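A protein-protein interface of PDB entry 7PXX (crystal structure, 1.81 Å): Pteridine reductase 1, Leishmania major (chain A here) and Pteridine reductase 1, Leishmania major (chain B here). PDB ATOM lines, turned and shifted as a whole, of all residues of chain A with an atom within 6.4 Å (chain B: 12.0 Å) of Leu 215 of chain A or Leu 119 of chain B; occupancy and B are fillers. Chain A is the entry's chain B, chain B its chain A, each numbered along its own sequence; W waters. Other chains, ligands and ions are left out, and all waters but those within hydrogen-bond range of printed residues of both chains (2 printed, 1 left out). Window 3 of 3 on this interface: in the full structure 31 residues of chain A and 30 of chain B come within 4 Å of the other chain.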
ATOM      1  N   LYS A 156      20.635 -14.746   7.774  1.00  0.00           N
ATOM      2  CA  LYS A 156      19.848 -15.139   6.615  1.00  0.00           C
ATOM      3  C   LYS A 156      20.718 -15.205   5.362  1.00  0.00           C
ATOM      4  O   LYS A 156      20.653 -16.170   4.594  1.00  0.00           O
ATOM      5  CB  LYS A 156      18.698 -14.151   6.434  1.00  0.00           C
ATOM      6  CG  LYS A 156      17.613 -14.595   5.484  1.00  0.00           C
ATOM      7  CD  LYS A 156      16.637 -13.463   5.260  1.00  0.00           C
ATOM      8  CE  LYS A 156      15.204 -13.934   5.326  1.00  0.00           C
ATOM      9  NZ  LYS A 156      14.284 -12.794   5.089  1.00  0.00           N
ATOM     10  N   ALA A 159      23.270 -18.122   5.638  1.00  0.00           N
ATOM     11  CA  ALA A 159      22.639 -19.433   5.499  1.00  0.00           C
ATOM     12  C   ALA A 159      22.115 -19.660   4.085  1.00  0.00           C
ATOM     13  O   ALA A 159      22.138 -20.789   3.574  1.00  0.00           O
ATOM     14  CB  ALA A 159      21.500 -19.569   6.510  1.00  0.00           C
ATOM     15  N   HIS A 160      21.583 -18.612   3.460  1.00  0.00           N
ATOM     16  CA  HIS A 160      21.190 -18.719   2.061  1.00  0.00           C
ATOM     17  C   HIS A 160      22.364 -19.155   1.198  1.00  0.00           C
ATOM     18  O   HIS A 160      22.186 -19.905   0.236  1.00  0.00           O
ATOM     19  CB  HIS A 160      20.646 -17.382   1.555  1.00  0.00           C
ATOM     20  CG  HIS A 160      19.201 -17.149   1.868  1.00  0.00           C
ATOM     21  ND1 HIS A 160      18.564 -17.715   2.953  1.00  0.00           N
ATOM     22  CD2 HIS A 160      18.265 -16.411   1.226  1.00  0.00           C
ATOM     23  CE1 HIS A 160      17.298 -17.335   2.962  1.00  0.00           C
ATOM     24  NE2 HIS A 160      17.091 -16.545   1.926  1.00  0.00           N
ATOM     25  N   VAL A 162      25.145 -20.925   2.052  1.00  0.00           N
ATOM     26  CA  VAL A 162      25.426 -22.338   2.274  1.00  0.00           C
ATOM     27  C   VAL A 162      24.404 -23.195   1.542  1.00  0.00           C
ATOM     28  O   VAL A 162      24.759 -24.165   0.860  1.00  0.00           O
ATOM     29  CB  VAL A 162      25.453 -22.657   3.776  1.00  0.00           C
ATOM     30  CG1 VAL A 162      25.901 -24.096   3.999  1.00  0.00           C
ATOM     31  CG2 VAL A 162      26.409 -21.711   4.499  1.00  0.00           C
ATOM     32  N   ALA A 163      23.118 -22.842   1.667  1.00  0.00           N
ATOM     33  CA  ALA A 163      22.072 -23.602   0.991  1.00  0.00           C
ATOM     34  C   ALA A 163      22.273 -23.596  -0.520  1.00  0.00           C
ATOM     35  O   ALA A 163      22.076 -24.622  -1.180  1.00  0.00           O
ATOM     36  CB  ALA A 163      20.694 -23.046   1.355  1.00  0.00           C
ATOM     37  N   ARG A 170      30.375 -27.549  -0.022  1.00  0.00           N
ATOM     38  CA  ARG A 170      30.232 -26.868   1.259  1.00  0.00           C
ATOM     39  C   ARG A 170      31.450 -27.126   2.139  1.00  0.00           C
ATOM     40  O   ARG A 170      32.099 -28.172   2.053  1.00  0.00           O
ATOM     41  CB  ARG A 170      28.960 -27.328   1.978  1.00  0.00           C
ATOM     42  CG  ARG A 170      27.667 -27.074   1.187  1.00  0.00           C
ATOM     43  CD  ARG A 170      26.414 -27.468   1.963  1.00  0.00           C
ATOM     44  NE  ARG A 170      25.203 -27.164   1.209  1.00  0.00           N
ATOM     45  CZ  ARG A 170      24.069 -27.842   1.321  1.00  0.00           C
ATOM     46  NH1 ARG A 170      23.994 -28.870   2.162  1.00  0.00           N
ATOM     47  NH2 ARG A 170      23.007 -27.496   0.595  1.00  0.00           N
ATOM     48  N   GLY A 171      31.762 -26.152   2.982  1.00  0.00           N
ATOM     49  CA  GLY A 171      32.777 -26.338   3.993  1.00  0.00           C
ATOM     50  C   GLY A 171      32.313 -27.288   5.084  1.00  0.00           C
ATOM     51  O   GLY A 171      31.146 -27.658   5.190  1.00  0.00           O
ATOM     52  N   TYR A 174      30.921 -24.751   9.503  1.00  0.00           N
ATOM     53  CA  TYR A 174      30.252 -23.457   9.518  1.00  0.00           C
ATOM     54  C   TYR A 174      29.927 -23.077  10.955  1.00  0.00           C
ATOM     55  O   TYR A 174      29.379 -23.885  11.709  1.00  0.00           O
ATOM     56  CB  TYR A 174      28.970 -23.493   8.686  1.00  0.00           C
ATOM     57  CG  TYR A 174      29.186 -23.592   7.203  1.00  0.00           C
ATOM     58  CD1 TYR A 174      29.635 -22.495   6.463  1.00  0.00           C
ATOM     59  CD2 TYR A 174      28.928 -24.778   6.531  1.00  0.00           C
ATOM     60  CE1 TYR A 174      29.822 -22.584   5.092  1.00  0.00           C
ATOM     61  CE2 TYR A 174      29.111 -24.875   5.164  1.00  0.00           C
ATOM     62  CZ  TYR A 174      29.561 -23.779   4.452  1.00  0.00           C
ATOM     63  OH  TYR A 174      29.742 -23.890   3.093  1.00  0.00           O
ATOM     64  N   GLU A 211      17.158 -23.771  13.539  1.00  0.00           N
ATOM     65  CA  GLU A 211      16.703 -23.810  12.156  1.00  0.00           C
ATOM     66  C   GLU A 211      17.824 -24.208  11.197  1.00  0.00           C
ATOM     67  O   GLU A 211      17.557 -24.826  10.157  1.00  0.00           O
ATOM     68  CB  GLU A 211      16.102 -22.458  11.767  1.00  0.00           C
ATOM     69  CG  GLU A 211      15.427 -22.483  10.410  1.00  0.00           C
ATOM     70  CD  GLU A 211      14.433 -21.346  10.187  1.00  0.00           C
ATOM     71  OE1 GLU A 211      13.973 -20.696  11.165  1.00  0.00           O
ATOM     72  OE2 GLU A 211      14.096 -21.117   9.005  1.00  0.00           O
ATOM     73  N   LEU A 212      19.068 -23.889  11.527  1.00  0.00           N
ATOM     74  CA  LEU A 212      20.184 -24.118  10.621  1.00  0.00           C
ATOM     75  C   LEU A 212      20.959 -25.384  10.957  1.00  0.00           C
ATOM     76  O   LEU A 212      21.892 -25.729  10.232  1.00  0.00           O
ATOM     77  CB  LEU A 212      21.126 -22.905  10.621  1.00  0.00           C
ATOM     78  CG  LEU A 212      20.511 -21.542  10.289  1.00  0.00           C
ATOM     79  CD1 LEU A 212      21.589 -20.456  10.275  1.00  0.00           C
ATOM     80  CD2 LEU A 212      19.755 -21.556   8.966  1.00  0.00           C
ATOM     81  N   ALA A 213      20.572 -26.093  12.015  1.00  0.00           N
ATOM     82  CA  ALA A 213      21.184 -27.385  12.318  1.00  0.00           C
ATOM     83  C   ALA A 213      21.229 -28.365  11.150  1.00  0.00           C
ATOM     84  O   ALA A 213      22.233 -29.087  11.044  1.00  0.00           O
ATOM     85  CB  ALA A 213      20.455 -28.046  13.498  1.00  0.00           C
ATOM     86  N   PRO A 214      20.208 -28.492  10.287  1.00  0.00           N
ATOM     87  CA  PRO A 214      20.310 -29.471   9.185  1.00  0.00           C
ATOM     88  C   PRO A 214      21.370 -29.116   8.164  1.00  0.00           C
ATOM     89  O   PRO A 214      21.851 -30.013   7.461  1.00  0.00           O
ATOM     90  CB  PRO A 214      18.910 -29.460   8.553  1.00  0.00           C
ATOM     91  CG  PRO A 214      18.010 -28.911   9.635  1.00  0.00           C
ATOM     92  CD  PRO A 214      18.860 -27.898  10.351  1.00  0.00           C
ATOM     93  N   LEU A 215      21.748 -27.847   8.063  1.00  0.00           N
ATOM     94  CA  LEU A 215      22.888 -27.437   7.263  1.00  0.00           C
ATOM     95  C   LEU A 215      24.206 -27.563   8.006  1.00  0.00           C
ATOM     96  O   LEU A 215      25.251 -27.242   7.434  1.00  0.00           O
ATOM     97  CB  LEU A 215      22.690 -25.998   6.787  1.00  0.00           C
ATOM     98  CG  LEU A 215      21.659 -25.857   5.667  1.00  0.00           C
ATOM     99  CD1 LEU A 215      21.254 -24.405   5.513  1.00  0.00           C
ATOM    100  CD2 LEU A 215      22.202 -26.441   4.333  1.00  0.00           C
ATOM    101  N   GLN A 216      24.182 -28.047   9.248  1.00  0.00           N
ATOM    102  CA  GLN A 216      25.363 -28.148  10.108  1.00  0.00           C
ATOM    103  C   GLN A 216      26.002 -26.781  10.368  1.00  0.00           C
ATOM    104  O   GLN A 216      27.210 -26.680  10.619  1.00  0.00           O
ATOM    105  CB  GLN A 216      26.386 -29.139   9.542  1.00  0.00           C
ATOM    106  CG  GLN A 216      25.877 -30.579   9.516  1.00  0.00           C
ATOM    107  CD  GLN A 216      26.862 -31.537   8.874  1.00  0.00           C
ATOM    108  OE1 GLN A 216      27.923 -31.130   8.391  1.00  0.00           O
ATOM    109  NE2 GLN A 216      26.518 -32.818   8.863  1.00  0.00           N
ATOM    110  N   ILE A 217      25.196 -25.717  10.336  1.00  0.00           N
ATOM    111  CA  ILE A 217      25.640 -24.396  10.762  1.00  0.00           C
ATOM    112  C   ILE A 217      25.383 -24.276  12.257  1.00  0.00           C
ATOM    113  O   ILE A 217      24.233 -24.337  12.707  1.00  0.00           O
ATOM    114  CB  ILE A 217      24.917 -23.280   9.993  1.00  0.00           C
ATOM    115  CG1 ILE A 217      25.175 -23.394   8.483  1.00  0.00           C
ATOM    116  CG2 ILE A 217      25.376 -21.926  10.501  1.00  0.00           C
ATOM    117  CD1 ILE A 217      24.438 -22.351   7.660  1.00  0.00           C
ATOM    118  N   PRO B 115       5.420 -16.885  10.646  1.00  0.00           N
ATOM    119  CA  PRO B 115       6.804 -17.303  10.410  1.00  0.00           C
ATOM    120  C   PRO B 115       7.616 -16.275   9.654  1.00  0.00           C
ATOM    121  O   PRO B 115       7.095 -15.523   8.824  1.00  0.00           O
ATOM    122  CB  PRO B 115       6.657 -18.581   9.568  1.00  0.00           C
ATOM    123  CG  PRO B 115       5.256 -19.028   9.782  1.00  0.00           C
ATOM    124  CD  PRO B 115       4.471 -17.769   9.947  1.00  0.00           C
ATOM    125  N   THR B 116       8.923 -16.292   9.932  1.00  0.00           N
ATOM    126  CA  THR B 116       9.957 -15.671   9.103  1.00  0.00           C
ATOM    127  C   THR B 116      11.090 -16.672   8.926  1.00  0.00           C
ATOM    128  O   THR B 116      12.143 -16.545   9.562  1.00  0.00           O
ATOM    129  CB  THR B 116      10.501 -14.395   9.737  1.00  0.00           C
ATOM    130  OG1 THR B 116      10.902 -14.689  11.079  1.00  0.00           O
ATOM    131  CG2 THR B 116       9.424 -13.339   9.768  1.00  0.00           C
ATOM    132  N   PRO B 117      10.937 -17.642   8.026  1.00  0.00           N
ATOM    133  CA  PRO B 117      11.944 -18.700   7.904  1.00  0.00           C
ATOM    134  C   PRO B 117      13.287 -18.155   7.434  1.00  0.00           C
ATOM    135  O   PRO B 117      13.369 -17.251   6.599  1.00  0.00           O
ATOM    136  CB  PRO B 117      11.341 -19.657   6.865  1.00  0.00           C
ATOM    137  CG  PRO B 117       9.913 -19.244   6.705  1.00  0.00           C
ATOM    138  CD  PRO B 117       9.858 -17.790   7.041  1.00  0.00           C
ATOM    139  N   LEU B 118      14.358 -18.727   7.974  1.00  0.00           N
ATOM    140  CA  LEU B 118      15.677 -18.272   7.565  1.00  0.00           C
ATOM    141  C   LEU B 118      16.072 -18.806   6.205  1.00  0.00           C
ATOM    142  O   LEU B 118      16.970 -18.238   5.578  1.00  0.00           O
ATOM    143  CB  LEU B 118      16.720 -18.679   8.595  1.00  0.00           C
ATOM    144  CG  LEU B 118      16.760 -17.754   9.811  1.00  0.00           C
ATOM    145  CD1 LEU B 118      17.595 -18.375  10.931  1.00  0.00           C
ATOM    146  CD2 LEU B 118      17.309 -16.401   9.400  1.00  0.00           C
ATOM    147  N   LEU B 119      15.421 -19.870   5.735  1.00  0.00           N
ATOM    148  CA  LEU B 119      15.760 -20.494   4.468  1.00  0.00           C
ATOM    149  C   LEU B 119      14.542 -20.559   3.556  1.00  0.00           C
ATOM    150  O   LEU B 119      13.404 -20.704   4.015  1.00  0.00           O
ATOM    151  CB  LEU B 119      16.328 -21.894   4.686  1.00  0.00           C
ATOM    152  CG  LEU B 119      17.498 -21.892   5.660  1.00  0.00           C
ATOM    153  CD1 LEU B 119      17.743 -23.273   6.248  1.00  0.00           C
ATOM    154  CD2 LEU B 119      18.725 -21.346   4.977  1.00  0.00           C
ATOM    155  N   ARG B 120      14.807 -20.450   2.255  1.00  0.00           N
ATOM    156  CA  ARG B 120      13.778 -20.505   1.222  1.00  0.00           C
ATOM    157  C   ARG B 120      14.384 -20.943  -0.107  1.00  0.00           C
ATOM    158  O   ARG B 120      15.096 -20.173  -0.757  1.00  0.00           O
ATOM    159  CB  ARG B 120      13.099 -19.145   1.063  1.00  0.00           C
ATOM    160  N   MET B 136       9.261  -8.250   3.271  1.00  0.00           N
ATOM    161  CA  MET B 136      10.300  -8.559   4.243  1.00  0.00           C
ATOM    162  C   MET B 136      10.402  -7.458   5.289  1.00  0.00           C
ATOM    163  O   MET B 136      10.429  -7.736   6.496  1.00  0.00           O
ATOM    164  CB  MET B 136      11.642  -8.757   3.533  1.00  0.00           C
ATOM    165  N   LEU B 188      10.216 -21.838  18.420  1.00  0.00           N
ATOM    166  CA  LEU B 188       9.325 -22.392  17.420  1.00  0.00           C
ATOM    167  C   LEU B 188      10.014 -22.320  16.067  1.00  0.00           C
ATOM    168  O   LEU B 188      10.489 -21.254  15.668  1.00  0.00           O
ATOM    169  CB  LEU B 188       8.003 -21.619  17.397  1.00  0.00           C
ATOM    170  CG  LEU B 188       6.844 -22.218  16.594  1.00  0.00           C
ATOM    171  CD1 LEU B 188       6.489 -23.617  17.096  1.00  0.00           C
ATOM    172  CD2 LEU B 188       5.613 -21.272  16.624  1.00  0.00           C
ATOM    173  N   LEU B 189      10.074 -23.450  15.373  1.00  0.00           N
ATOM    174  CA  LEU B 189      10.820 -23.532  14.118  1.00  0.00           C
ATOM    175  C   LEU B 189      10.253 -22.585  13.062  1.00  0.00           C
ATOM    176  O   LEU B 189       9.064 -22.627  12.742  1.00  0.00           O
ATOM    177  CB  LEU B 189      10.795 -24.959  13.606  1.00  0.00           C
ATOM    178  CG  LEU B 189      11.651 -25.265  12.386  1.00  0.00           C
ATOM    179  CD1 LEU B 189      13.101 -25.041  12.731  1.00  0.00           C
ATOM    180  CD2 LEU B 189      11.399 -26.707  11.931  1.00  0.00           C
ATOM    181  N   GLY B 190      11.109 -21.723  12.525  1.00  0.00           N
ATOM    182  CA  GLY B 190      10.717 -20.804  11.473  1.00  0.00           C
ATOM    183  C   GLY B 190      10.210 -19.451  11.937  1.00  0.00           C
ATOM    184  O   GLY B 190       9.855 -18.617  11.089  1.00  0.00           O
ATOM    185  N   TYR B 191      10.178 -19.198  13.241  1.00  0.00           N
ATOM    186  CA  TYR B 191       9.594 -17.982  13.801  1.00  0.00           C
ATOM    187  C   TYR B 191      10.643 -17.027  14.382  1.00  0.00           C
ATOM    188  O   TYR B 191      10.413 -16.429  15.433  1.00  0.00           O
ATOM    189  CB  TYR B 191       8.571 -18.334  14.877  1.00  0.00           C
ATOM    190  CG  TYR B 191       7.226 -18.795  14.332  1.00  0.00           C
ATOM    191  CD1 TYR B 191       7.101 -20.016  13.690  1.00  0.00           C
ATOM    192  CD2 TYR B 191       6.092 -18.006  14.471  1.00  0.00           C
ATOM    193  CE1 TYR B 191       5.872 -20.444  13.200  1.00  0.00           C
ATOM    194  CE2 TYR B 191       4.858 -18.416  13.976  1.00  0.00           C
ATOM    195  CZ  TYR B 191       4.754 -19.633  13.337  1.00  0.00           C
ATOM    196  OH  TYR B 191       3.527 -20.058  12.840  1.00  0.00           O
ATOM    197  N   THR B 192      11.764 -16.810  13.662  1.00  0.00           N
ATOM    198  CA  THR B 192      12.934 -16.147  14.251  1.00  0.00           C
ATOM    199  C   THR B 192      12.647 -14.710  14.686  1.00  0.00           C
ATOM    200  O   THR B 192      13.101 -14.279  15.758  1.00  0.00           O
ATOM    201  CB  THR B 192      14.127 -16.197  13.279  1.00  0.00           C
ATOM    202  OG1 THR B 192      14.604 -17.542  13.195  1.00  0.00           O
ATOM    203  CG2 THR B 192      15.304 -15.325  13.767  1.00  0.00           C
ATOM    204  N   ILE B 193      11.921 -13.929  13.879  1.00  0.00           N
ATOM    205  CA  ILE B 193      11.693 -12.550  14.302  1.00  0.00           C
ATOM    206  C   ILE B 193      10.794 -12.500  15.525  1.00  0.00           C
ATOM    207  O   ILE B 193      11.029 -11.721  16.445  1.00  0.00           O
ATOM    208  CB  ILE B 193      11.124 -11.692  13.161  1.00  0.00           C
ATOM    209  CG1 ILE B 193      12.080 -11.700  11.973  1.00  0.00           C
ATOM    210  CG2 ILE B 193      10.974 -10.251  13.636  1.00  0.00           C
ATOM    211  CD1 ILE B 193      13.331 -10.923  12.219  1.00  0.00           C
HETATM  212  O   HOH W   1      13.798 -20.934  13.770  1.00  0.00           O
HETATM  213  O   HOH W   2      12.375 -14.996   6.870  1.00  0.00           O
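Water W2 lies within hydrogen-bond range of O of Pro 117 of chain B, O of Thr 116 of chain B and NZ of Lys 156 of chain A.
Water W1 lies within hydrogen-bond range of the side-chain carboxylate of Glu 211 of chain A and the backbone NH of Gly 190 of chain B.
Leu 215 of chain A touches one residue of chain B.
Leu 119 of chain B touches just these residues of chain A: Ala 159 (3.6 Å), His 160 (3.8 Å), Glu 211 (3.7 Å), Leu 212 (3.8 Å) and Leu 215 (3.8 Å).
Ala 159 of chain A touches one residue of chain B.
No residue of chain B comes within 4 Å of Val 162 of chain A.
No residue of chain B comes within 4 Å of Ala 163 of chain A.
No residue of chain B comes within 4 Å of Tyr 174 of chain A.
Of chain B, only Pro 117 (3.4 Å), Leu 118 (2.6 Å), Leu 119 (3.7 Å), Leu 189 (3.8 Å), Gly 190 (3.3 Å) and Thr 192 (3.8 Å) come within 4 Å of Glu 211 of chain A.
No residue of chain B comes within 4 Å of Ala 213 of chain A.
No residue of chain B comes within 4 Å of Gln 216 of chain A.
No residue of chain B comes within 4 Å of Ile 217 of chain A.
Of the printed residues of chain A, Leu 189 of chain B touches Glu 211.
Of the printed residues of chain A, Gly 190 of chain B touches Glu 211 (3.3 Å).
Printed residues of chain B within 4 Å of Lys 156 of chain A: Pro 117 and Leu 118.
Printed residues of chain A within 4 Å of Leu 118 of chain B: Lys 156 (3.7 Å), His 160 (2.8 Å) and Glu 211 (2.6 Å).
Arg 170 of chain A touches none of the printed residues of chain B.
Leu 188 of chain B touches none of the printed residues of chain A.
The nearest residue of chain B that does not touch Leu 215 of chain A is Leu 118 of chain B (7.5 Å).
The nearest printed residue of chain A that does not touch Leu 118 of chain B is Leu 212 of chain A (4.2 Å).
The backbone NH (N) of Thr 116 of chain B is in hydrogen-bond range of the backbone carbonyl oxygen (O) of Gly 190 of chain B, at 2.8 Å.
N of Thr 192 of chain B sits at hydrogen-bond distance from OG1 of Thr 116 of chain B, at 3.5 Å.
O of Lys 156 of chain A is in hydrogen-bond range of ND1 of His 160 of chain A.
The backbone carbonyl oxygen (O) of Leu 212 of chain A lies within hydrogen-bond range of the backbone NH (N) of Ile 217 of chain A, 3.3 Å away.
CE of Lys 156 of chain A touches O of Pro 117 of chain B (3.999 Å).
Lys 156 of chain A touches Leu 118 of chain B (CG to O, 3.7 Å).
CB of Ala 159 of chain A touches CD2 of Leu 119 of chain B (3.6 Å).
CE1 of His 160 of chain A touches CA of Leu 119 of chain B, 3.8 Å away.
Glu 211 of chain A touches Pro 117 of chain B.
Glu 211 of chain A touches Leu 119 of chain B.
CD1 of Leu 189 of chain B touches CA of Glu 211 of chain A, at 3.8 Å.
Glu 211 of chain A touches Thr 192 of chain B (OE1 to OG1, 3.8 Å).
Leu 212 of chain A touches Leu 119 of chain B.
Leu 119 of chain B touches Leu 215 of chain A.
A ring nitrogen (ND1) of His 160 of chain A lies close to the backbone carbonyl oxygen (O) of Leu 118 of chain B (3.1 Å).
The side-chain carboxylate of Glu 211 of chain A sits at hydrogen-bond distance from the backbone NH of Leu 118 of chain B.
The backbone NH of Gly 190 of chain B lies close to the side-chain carboxylate of Glu 211 of chain A (3.3 Å).
Of the 15 printed residues of chain A, 6 touch a printed residue of chain B.
Hydrophobic or aromatic side chains of chain A that line the printed part of chain B: Ala 159, His 160, Leu 212 and Leu 215.
Along chain A the printed residues that touch a printed residue of chain B span positions 156 to 215.
Of the 13 printed residues of chain B, 6 touch a printed residue of chain A.
Hydrophobic or aromatic side chains of chain B that line the printed part of chain A: Pro 117, Leu 118, Leu 119 and Leu 189.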
